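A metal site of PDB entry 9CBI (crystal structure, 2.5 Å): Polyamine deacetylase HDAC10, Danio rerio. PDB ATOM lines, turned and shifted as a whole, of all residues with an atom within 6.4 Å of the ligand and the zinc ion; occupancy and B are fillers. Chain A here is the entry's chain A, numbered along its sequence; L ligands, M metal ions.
CG of Glu 24 touches C7 of the ligand, 3.6 Å away. CB of Ala 94 touches C7 of the ligand, at 3.7 Å. NE2 of His 137 touches C1 of the ligand, at 3.4 Å. Gly 145 touches the ligand. Phe 146 touches the ligand (CE2 to C10, 3.4 Å). CZ3 of Trp 205 touches C4 of the ligand, at 3.5 Å. Gly 305 touches the ligand (CA to S1, 3.9 Å). Hydrophobic or aromatic side chains within 4 Å of the ligand: Ala 94, His 137, Phe 146, His 176, Trp 205 and Tyr 307. 13 residues have an atom within 4 Å of the ligand: Glu 24, Ala 94, His 136, His 137, Gly 145, Phe 146, Asp 174, His 176, Trp 205, Asp 267, Glu 274, Gly 305 and Tyr 307.
OE2 of Glu 274 is in salt-bridge range of N1 of the ligand (2.7 Å). S1 of the ligand lies close to NE2 of His 136 (3.4 Å). OH of Tyr 307 is in hydrogen-bond range of O1 of the ligand (2.8 Å).
NE1 of Trp 205 is in hydrogen-bond range of OD1 of Asn 93 (2.8 Å). SG of Cys 147 lies within hydrogen-bond range of O of Gly 145 (3.2 Å). A ring nitrogen (NE2) of His 137 lies within hydrogen-bond range of a ring nitrogen (NE2) of His 136, at 3.0 Å. N of Val 175 is in hydrogen-bond range of OD1 of Asp 267 (3.0 Å). The backbone NH (N) of His 136 sits at hydrogen-bond distance from the side-chain sulfur (SG) of Cys 147 (3.8 Å). The side-chain sulfur (SG) of Cys 147 sits at hydrogen-bond distance from the backbone NH (N) of His 137, at 3.6 Å. The backbone carbonyl oxygen (O) of Ala 94 is in hydrogen-bond range of the backbone NH (N) of Phe 146, at 2.9 Å. O of Asn 93 lies within hydrogen-bond range of N of Gly 145, 3.3 Å away.
The zinc ion is bound by the side-chain carboxylate (OD2) of Asp 267 (2.0 Å), the side-chain carboxylate (OD1) of Asp 174 (2.2 Å), a ring nitrogen (ND1) of His 176 (2.3 Å) and a sulfur (S1) of the ligand (2.4 Å). The zinc ion has four donor atoms within binding distance. Slightly farther from the zinc ion lies OD2 of Asp 174 (2.8 Å). Slightly farther from the zinc ion lies O1 of the ligand (2.8 Å).
Of the 24 residues printed, 3 come within 4 Å of the zinc ion. Along chain A the residues within 4 Å of the zinc ion span positions 174 to 267.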
ATOM      1  N   GLU A  24      25.151   6.417 -20.303  1.00  0.00           N
ATOM      2  CA  GLU A  24      24.876   6.469 -18.869  1.00  0.00           C
ATOM      3  C   GLU A  24      25.710   5.450 -18.096  1.00  0.00           C
ATOM      4  O   GLU A  24      25.998   5.666 -16.909  1.00  0.00           O
ATOM      5  CB  GLU A  24      23.387   6.232 -18.610  1.00  0.00           C
ATOM      6  CG  GLU A  24      22.745   7.270 -17.698  1.00  0.00           C
ATOM      7  CD  GLU A  24      21.248   7.063 -17.543  1.00  0.00           C
ATOM      8  N   CYS A  25      26.104   4.341 -18.730  1.00  0.00           N
ATOM      9  CA  CYS A  25      26.812   3.258 -18.054  1.00  0.00           C
ATOM     10  C   CYS A  25      28.241   3.071 -18.523  1.00  0.00           C
ATOM     11  O   CYS A  25      28.908   2.133 -18.066  1.00  0.00           O
ATOM     12  CB  CYS A  25      26.041   1.942 -18.240  1.00  0.00           C
ATOM     13  SG  CYS A  25      24.329   1.957 -17.677  1.00  0.00           S
ATOM     14  N   ILE A  27      30.890   4.348 -17.720  1.00  0.00           N
ATOM     15  CA  ILE A  27      31.927   4.508 -16.697  1.00  0.00           C
ATOM     16  C   ILE A  27      32.177   3.221 -15.933  1.00  0.00           C
ATOM     17  O   ILE A  27      33.309   2.952 -15.506  1.00  0.00           O
ATOM     18  CB  ILE A  27      31.566   5.651 -15.743  1.00  0.00           C
ATOM     19  CG1 ILE A  27      30.157   5.453 -15.182  1.00  0.00           C
ATOM     20  CG2 ILE A  27      31.683   6.994 -16.446  1.00  0.00           C
ATOM     21  CD1 ILE A  27      29.759   6.477 -14.147  1.00  0.00           C
ATOM     22  N   ASN A  93      16.531   1.120 -14.808  1.00  0.00           N
ATOM     23  CA  ASN A  93      17.099   2.463 -14.893  1.00  0.00           C
ATOM     24  C   ASN A  93      18.586   2.439 -14.596  1.00  0.00           C
ATOM     25  O   ASN A  93      18.997   2.013 -13.509  1.00  0.00           O
ATOM     26  CB  ASN A  93      16.373   3.411 -13.936  1.00  0.00           C
ATOM     27  CG  ASN A  93      16.861   4.848 -14.066  1.00  0.00           C
ATOM     28  OD1 ASN A  93      17.591   5.346 -13.213  1.00  0.00           O
ATOM     29  ND2 ASN A  93      16.457   5.519 -15.143  1.00  0.00           N
ATOM     30  N   ALA A  94      19.390   2.896 -15.559  1.00  0.00           N
ATOM     31  CA  ALA A  94      20.833   3.103 -15.377  1.00  0.00           C
ATOM     32  C   ALA A  94      21.551   1.807 -15.013  1.00  0.00           C
ATOM     33  O   ALA A  94      22.438   1.784 -14.162  1.00  0.00           O
ATOM     34  CB  ALA A  94      21.118   4.192 -14.339  1.00  0.00           C
ATOM     35  N   PRO A 134      28.253  -3.122  -7.856  1.00  0.00           N
ATOM     36  CA  PRO A 134      27.881  -2.529  -6.559  1.00  0.00           C
ATOM     37  C   PRO A 134      26.473  -2.930  -6.161  1.00  0.00           C
ATOM     38  O   PRO A 134      25.808  -3.670  -6.891  1.00  0.00           O
ATOM     39  CB  PRO A 134      27.987  -1.024  -6.830  1.00  0.00           C
ATOM     40  CG  PRO A 134      27.761  -0.898  -8.297  1.00  0.00           C
ATOM     41  CD  PRO A 134      28.394  -2.113  -8.913  1.00  0.00           C
ATOM     42  N   HIS A 136      24.215  -0.787  -3.501  1.00  0.00           N
ATOM     43  CA  HIS A 136      23.384   0.051  -2.642  1.00  0.00           C
ATOM     44  C   HIS A 136      22.193   0.678  -3.361  1.00  0.00           C
ATOM     45  O   HIS A 136      21.313   1.229  -2.683  1.00  0.00           O
ATOM     46  CB  HIS A 136      24.224   1.131  -1.954  1.00  0.00           C
ATOM     47  CG  HIS A 136      24.771   2.176  -2.880  1.00  0.00           C
ATOM     48  ND1 HIS A 136      25.105   3.443  -2.457  1.00  0.00           N
ATOM     49  CD2 HIS A 136      25.073   2.136  -4.206  1.00  0.00           C
ATOM     50  CE1 HIS A 136      25.572   4.141  -3.475  1.00  0.00           C
ATOM     51  NE2 HIS A 136      25.559   3.377  -4.544  1.00  0.00           N
ATOM     52  N   HIS A 137      22.114   0.601  -4.681  1.00  0.00           N
ATOM     53  CA  HIS A 137      20.955   1.130  -5.387  1.00  0.00           C
ATOM     54  C   HIS A 137      19.895   0.077  -5.697  1.00  0.00           C
ATOM     55  O   HIS A 137      18.728   0.440  -5.887  1.00  0.00           O
ATOM     56  CB  HIS A 137      21.375   1.795  -6.705  1.00  0.00           C
ATOM     57  CG  HIS A 137      22.156   3.047  -6.527  1.00  0.00           C
ATOM     58  ND1 HIS A 137      21.616   4.188  -5.959  1.00  0.00           N
ATOM     59  CD2 HIS A 137      23.432   3.355  -6.847  1.00  0.00           C
ATOM     60  CE1 HIS A 137      22.542   5.140  -5.929  1.00  0.00           C
ATOM     61  NE2 HIS A 137      23.651   4.663  -6.474  1.00  0.00           N
ATOM     62  N   ASN A 144      19.167  -1.355 -10.306  1.00  0.00           N
ATOM     63  CA  ASN A 144      19.182   0.102 -10.365  1.00  0.00           C
ATOM     64  C   ASN A 144      20.608   0.605 -10.180  1.00  0.00           C
ATOM     65  O   ASN A 144      21.365   0.048  -9.377  1.00  0.00           O
ATOM     66  CB  ASN A 144      18.269   0.695  -9.294  1.00  0.00           C
ATOM     67  CG  ASN A 144      18.023   2.171  -9.479  1.00  0.00           C
ATOM     68  OD1 ASN A 144      18.707   3.007  -8.886  1.00  0.00           O
ATOM     69  ND2 ASN A 144      17.030   2.510 -10.300  1.00  0.00           N
ATOM     70  N   GLY A 145      20.963   1.657 -10.916  1.00  0.00           N
ATOM     71  CA  GLY A 145      22.246   2.322 -10.782  1.00  0.00           C
ATOM     72  C   GLY A 145      23.454   1.412 -10.709  1.00  0.00           C
ATOM     73  O   GLY A 145      24.171   1.398  -9.702  1.00  0.00           O
ATOM     74  N   PHE A 146      23.681   0.623 -11.762  1.00  0.00           N
ATOM     75  CA  PHE A 146      24.765  -0.335 -11.916  1.00  0.00           C
ATOM     76  C   PHE A 146      24.678  -1.503 -10.929  1.00  0.00           C
ATOM     77  O   PHE A 146      25.593  -2.334 -10.905  1.00  0.00           O
ATOM     78  CB  PHE A 146      26.163   0.292 -11.767  1.00  0.00           C
ATOM     79  CG  PHE A 146      26.374   1.524 -12.592  1.00  0.00           C
ATOM     80  CD1 PHE A 146      25.668   1.728 -13.775  1.00  0.00           C
ATOM     81  CD2 PHE A 146      27.290   2.486 -12.200  1.00  0.00           C
ATOM     82  CE1 PHE A 146      25.871   2.870 -14.527  1.00  0.00           C
ATOM     83  CE2 PHE A 146      27.496   3.622 -12.944  1.00  0.00           C
ATOM     84  CZ  PHE A 146      26.786   3.816 -14.119  1.00  0.00           C
ATOM     85  N   CYS A 147      23.631  -1.589 -10.119  1.00  0.00           N
ATOM     86  CA  CYS A 147      23.535  -2.593  -9.066  1.00  0.00           C
ATOM     87  C   CYS A 147      22.499  -3.645  -9.423  1.00  0.00           C
ATOM     88  O   CYS A 147      21.434  -3.331  -9.978  1.00  0.00           O
ATOM     89  CB  CYS A 147      23.184  -1.943  -7.730  1.00  0.00           C
ATOM     90  SG  CYS A 147      24.294  -0.605  -7.254  1.00  0.00           S
ATOM     91  N   ASP A 174      29.513   6.706  -0.561  1.00  0.00           N
ATOM     92  CA  ASP A 174      29.366   6.860  -1.996  1.00  0.00           C
ATOM     93  C   ASP A 174      28.674   8.187  -2.289  1.00  0.00           C
ATOM     94  O   ASP A 174      27.868   8.687  -1.499  1.00  0.00           O
ATOM     95  CB  ASP A 174      28.560   5.682  -2.570  1.00  0.00           C
ATOM     96  CG  ASP A 174      28.580   5.643  -4.084  1.00  0.00           C
ATOM     97  OD1 ASP A 174      28.044   6.574  -4.729  1.00  0.00           O
ATOM     98  OD2 ASP A 174      29.125   4.666  -4.640  1.00  0.00           O
ATOM     99  N   VAL A 175      28.995   8.781  -3.444  1.00  0.00           N
ATOM    100  CA  VAL A 175      28.435  10.080  -3.787  1.00  0.00           C
ATOM    101  C   VAL A 175      26.969  10.009  -4.165  1.00  0.00           C
ATOM    102  O   VAL A 175      26.310  11.049  -4.261  1.00  0.00           O
ATOM    103  CB  VAL A 175      29.241  10.739  -4.928  1.00  0.00           C
ATOM    104  CG1 VAL A 175      28.677  10.327  -6.290  1.00  0.00           C
ATOM    105  CG2 VAL A 175      29.245  12.260  -4.767  1.00  0.00           C
ATOM    106  N   HIS A 176      26.436   8.808  -4.384  1.00  0.00           N
ATOM    107  CA  HIS A 176      25.022   8.630  -4.674  1.00  0.00           C
ATOM    108  C   HIS A 176      24.290   8.122  -3.436  1.00  0.00           C
ATOM    109  O   HIS A 176      24.872   7.515  -2.536  1.00  0.00           O
ATOM    110  CB  HIS A 176      24.827   7.640  -5.829  1.00  0.00           C
ATOM    111  CG  HIS A 176      25.457   8.084  -7.113  1.00  0.00           C
ATOM    112  ND1 HIS A 176      26.769   7.818  -7.441  1.00  0.00           N
ATOM    113  CD2 HIS A 176      24.943   8.787  -8.159  1.00  0.00           C
ATOM    114  CE1 HIS A 176      27.044   8.322  -8.619  1.00  0.00           C
ATOM    115  NE2 HIS A 176      25.954   8.924  -9.085  1.00  0.00           N
ATOM    116  N   PHE A 204      19.864  15.952  -9.073  1.00  0.00           N
ATOM    117  CA  PHE A 204      20.867  14.955  -9.416  1.00  0.00           C
ATOM    118  C   PHE A 204      20.319  13.547  -9.179  1.00  0.00           C
ATOM    119  O   PHE A 204      19.513  13.316  -8.276  1.00  0.00           O
ATOM    120  CB  PHE A 204      22.150  15.152  -8.604  1.00  0.00           C
ATOM    121  CG  PHE A 204      23.287  14.279  -9.055  1.00  0.00           C
ATOM    122  CD1 PHE A 204      23.948  14.560 -10.240  1.00  0.00           C
ATOM    123  CD2 PHE A 204      23.697  13.196  -8.298  1.00  0.00           C
ATOM    124  CE1 PHE A 204      25.004  13.763 -10.670  1.00  0.00           C
ATOM    125  CE2 PHE A 204      24.751  12.401  -8.714  1.00  0.00           C
ATOM    126  CZ  PHE A 204      25.397  12.688  -9.902  1.00  0.00           C
ATOM    127  N   TRP A 205      20.781  12.620 -10.019  1.00  0.00           N
ATOM    128  CA  TRP A 205      20.310  11.246  -9.958  1.00  0.00           C
ATOM    129  C   TRP A 205      20.575  10.659  -8.567  1.00  0.00           C
ATOM    130  O   TRP A 205      21.640  10.887  -7.991  1.00  0.00           O
ATOM    131  CB  TRP A 205      21.019  10.407 -11.028  1.00  0.00           C
ATOM    132  CG  TRP A 205      20.402   9.067 -11.233  1.00  0.00           C
ATOM    133  CD1 TRP A 205      19.453   8.734 -12.152  1.00  0.00           C
ATOM    134  CD2 TRP A 205      20.684   7.872 -10.490  1.00  0.00           C
ATOM    135  NE1 TRP A 205      19.123   7.403 -12.026  1.00  0.00           N
ATOM    136  CE2 TRP A 205      19.870   6.856 -11.011  1.00  0.00           C
ATOM    137  CE3 TRP A 205      21.554   7.580  -9.434  1.00  0.00           C
ATOM    138  CZ2 TRP A 205      19.893   5.562 -10.515  1.00  0.00           C
ATOM    139  CZ3 TRP A 205      21.577   6.286  -8.939  1.00  0.00           C
ATOM    140  CH2 TRP A 205      20.748   5.292  -9.477  1.00  0.00           C
ATOM    141  N   GLY A 265      31.889   3.701  -1.621  1.00  0.00           N
ATOM    142  CA  GLY A 265      31.879   4.226  -2.962  1.00  0.00           C
ATOM    143  C   GLY A 265      32.797   5.429  -3.037  1.00  0.00           C
ATOM    144  O   GLY A 265      32.607   6.409  -2.322  1.00  0.00           O
ATOM    145  N   ASP A 267      33.336   7.391  -5.652  1.00  0.00           N
ATOM    146  CA  ASP A 267      32.964   8.458  -6.561  1.00  0.00           C
ATOM    147  C   ASP A 267      32.755   9.786  -5.848  1.00  0.00           C
ATOM    148  O   ASP A 267      32.462  10.792  -6.515  1.00  0.00           O
ATOM    149  CB  ASP A 267      31.702   8.078  -7.345  1.00  0.00           C
ATOM    150  CG  ASP A 267      30.631   7.464  -6.474  1.00  0.00           C
ATOM    151  OD1 ASP A 267      30.848   7.353  -5.244  1.00  0.00           O
ATOM    152  OD2 ASP A 267      29.582   7.077  -7.017  1.00  0.00           O
ATOM    153  N   GLU A 274      31.550  11.527 -12.025  1.00  0.00           N
ATOM    154  CA  GLU A 274      30.148  11.374 -11.653  1.00  0.00           C
ATOM    155  C   GLU A 274      29.780  12.165 -10.399  1.00  0.00           C
ATOM    156  O   GLU A 274      28.674  12.714 -10.325  1.00  0.00           O
ATOM    157  CB  GLU A 274      29.813   9.895 -11.441  1.00  0.00           C
ATOM    158  CG  GLU A 274      28.336   9.594 -11.353  1.00  0.00           C
ATOM    159  CD  GLU A 274      27.593   9.867 -12.652  1.00  0.00           C
ATOM    160  OE1 GLU A 274      28.234   9.818 -13.719  1.00  0.00           O
ATOM    161  OE2 GLU A 274      26.367  10.123 -12.594  1.00  0.00           O
ATOM    162  N   GLU A 304      31.672   0.191  -3.646  1.00  0.00           N
ATOM    163  CA  GLU A 304      30.491   0.599  -4.406  1.00  0.00           C
ATOM    164  C   GLU A 304      30.932   1.303  -5.683  1.00  0.00           C
ATOM    165  O   GLU A 304      31.468   0.666  -6.590  1.00  0.00           O
ATOM    166  CB  GLU A 304      29.584   1.492  -3.566  1.00  0.00           C
ATOM    167  CG  GLU A 304      29.072   0.852  -2.280  1.00  0.00           C
ATOM    168  CD  GLU A 304      27.862  -0.048  -2.504  1.00  0.00           C
ATOM    169  OE1 GLU A 304      27.344  -0.069  -3.632  1.00  0.00           O
ATOM    170  OE2 GLU A 304      27.436  -0.735  -1.548  1.00  0.00           O
ATOM    171  N   GLY A 305      30.728   2.618  -5.747  1.00  0.00           N
ATOM    172  CA  GLY A 305      31.100   3.398  -6.910  1.00  0.00           C
ATOM    173  C   GLY A 305      32.562   3.803  -6.890  1.00  0.00           C
ATOM    174  O   GLY A 305      33.381   3.313  -6.110  1.00  0.00           O
ATOM    175  N   GLY A 306      32.888   4.726  -7.794  1.00  0.00           N
ATOM    176  CA  GLY A 306      34.253   5.183  -7.987  1.00  0.00           C
ATOM    177  C   GLY A 306      34.755   4.871  -9.380  1.00  0.00           C
ATOM    178  O   GLY A 306      34.981   3.700  -9.715  1.00  0.00           O
ATOM    179  N   TYR A 307      34.941   5.900 -10.208  1.00  0.00           N
ATOM    180  CA  TYR A 307      35.133   5.691 -11.639  1.00  0.00           C
ATOM    181  C   TYR A 307      36.328   6.404 -12.252  1.00  0.00           C
ATOM    182  O   TYR A 307      36.658   6.121 -13.414  1.00  0.00           O
ATOM    183  CB  TYR A 307      33.859   6.075 -12.398  1.00  0.00           C
ATOM    184  CG  TYR A 307      32.661   5.383 -11.808  1.00  0.00           C
ATOM    185  CD1 TYR A 307      32.404   4.043 -12.096  1.00  0.00           C
ATOM    186  CD2 TYR A 307      31.812   6.027 -10.923  1.00  0.00           C
ATOM    187  CE1 TYR A 307      31.332   3.384 -11.542  1.00  0.00           C
ATOM    188  CE2 TYR A 307      30.727   5.385 -10.364  1.00  0.00           C
ATOM    189  CZ  TYR A 307      30.496   4.060 -10.680  1.00  0.00           C
ATOM    190  OH  TYR A 307      29.419   3.407 -10.120  1.00  0.00           O
HETATM  191  C1  LIG L   1      26.055   4.198  -8.763  1.00  0.00           C
HETATM  192  C2  LIG L   1      26.616   5.226  -9.743  1.00  0.00           C
HETATM  193  C3  LIG L   1      25.763   5.766 -10.866  1.00  0.00           C
HETATM  194  C4  LIG L   1      24.382   5.438 -10.938  1.00  0.00           C
HETATM  195  C5  LIG L   1      23.568   5.924 -11.974  1.00  0.00           C
HETATM  196  C6  LIG L   1      24.059   6.742 -13.002  1.00  0.00           C
HETATM  197  C7  LIG L   1      23.169   7.265 -14.120  1.00  0.00           C
HETATM  198  C8  LIG L   1      22.825   8.789 -14.118  1.00  0.00           C
HETATM  199  C9  LIG L   1      25.422   7.060 -12.917  1.00  0.00           C
HETATM  200  C10 LIG L   1      26.244   6.580 -11.881  1.00  0.00           C
HETATM  201  N1  LIG L   1      23.956   9.678 -13.828  1.00  0.00           N
HETATM  202  O1  LIG L   1      27.745   5.593  -9.612  1.00  0.00           O
HETATM  203  S1  LIG L   1      27.259   3.801  -7.417  1.00  0.00           S
HETATM  204 ZN    ZN M   1      27.967   5.962  -6.819  1.00  0.00          ZN
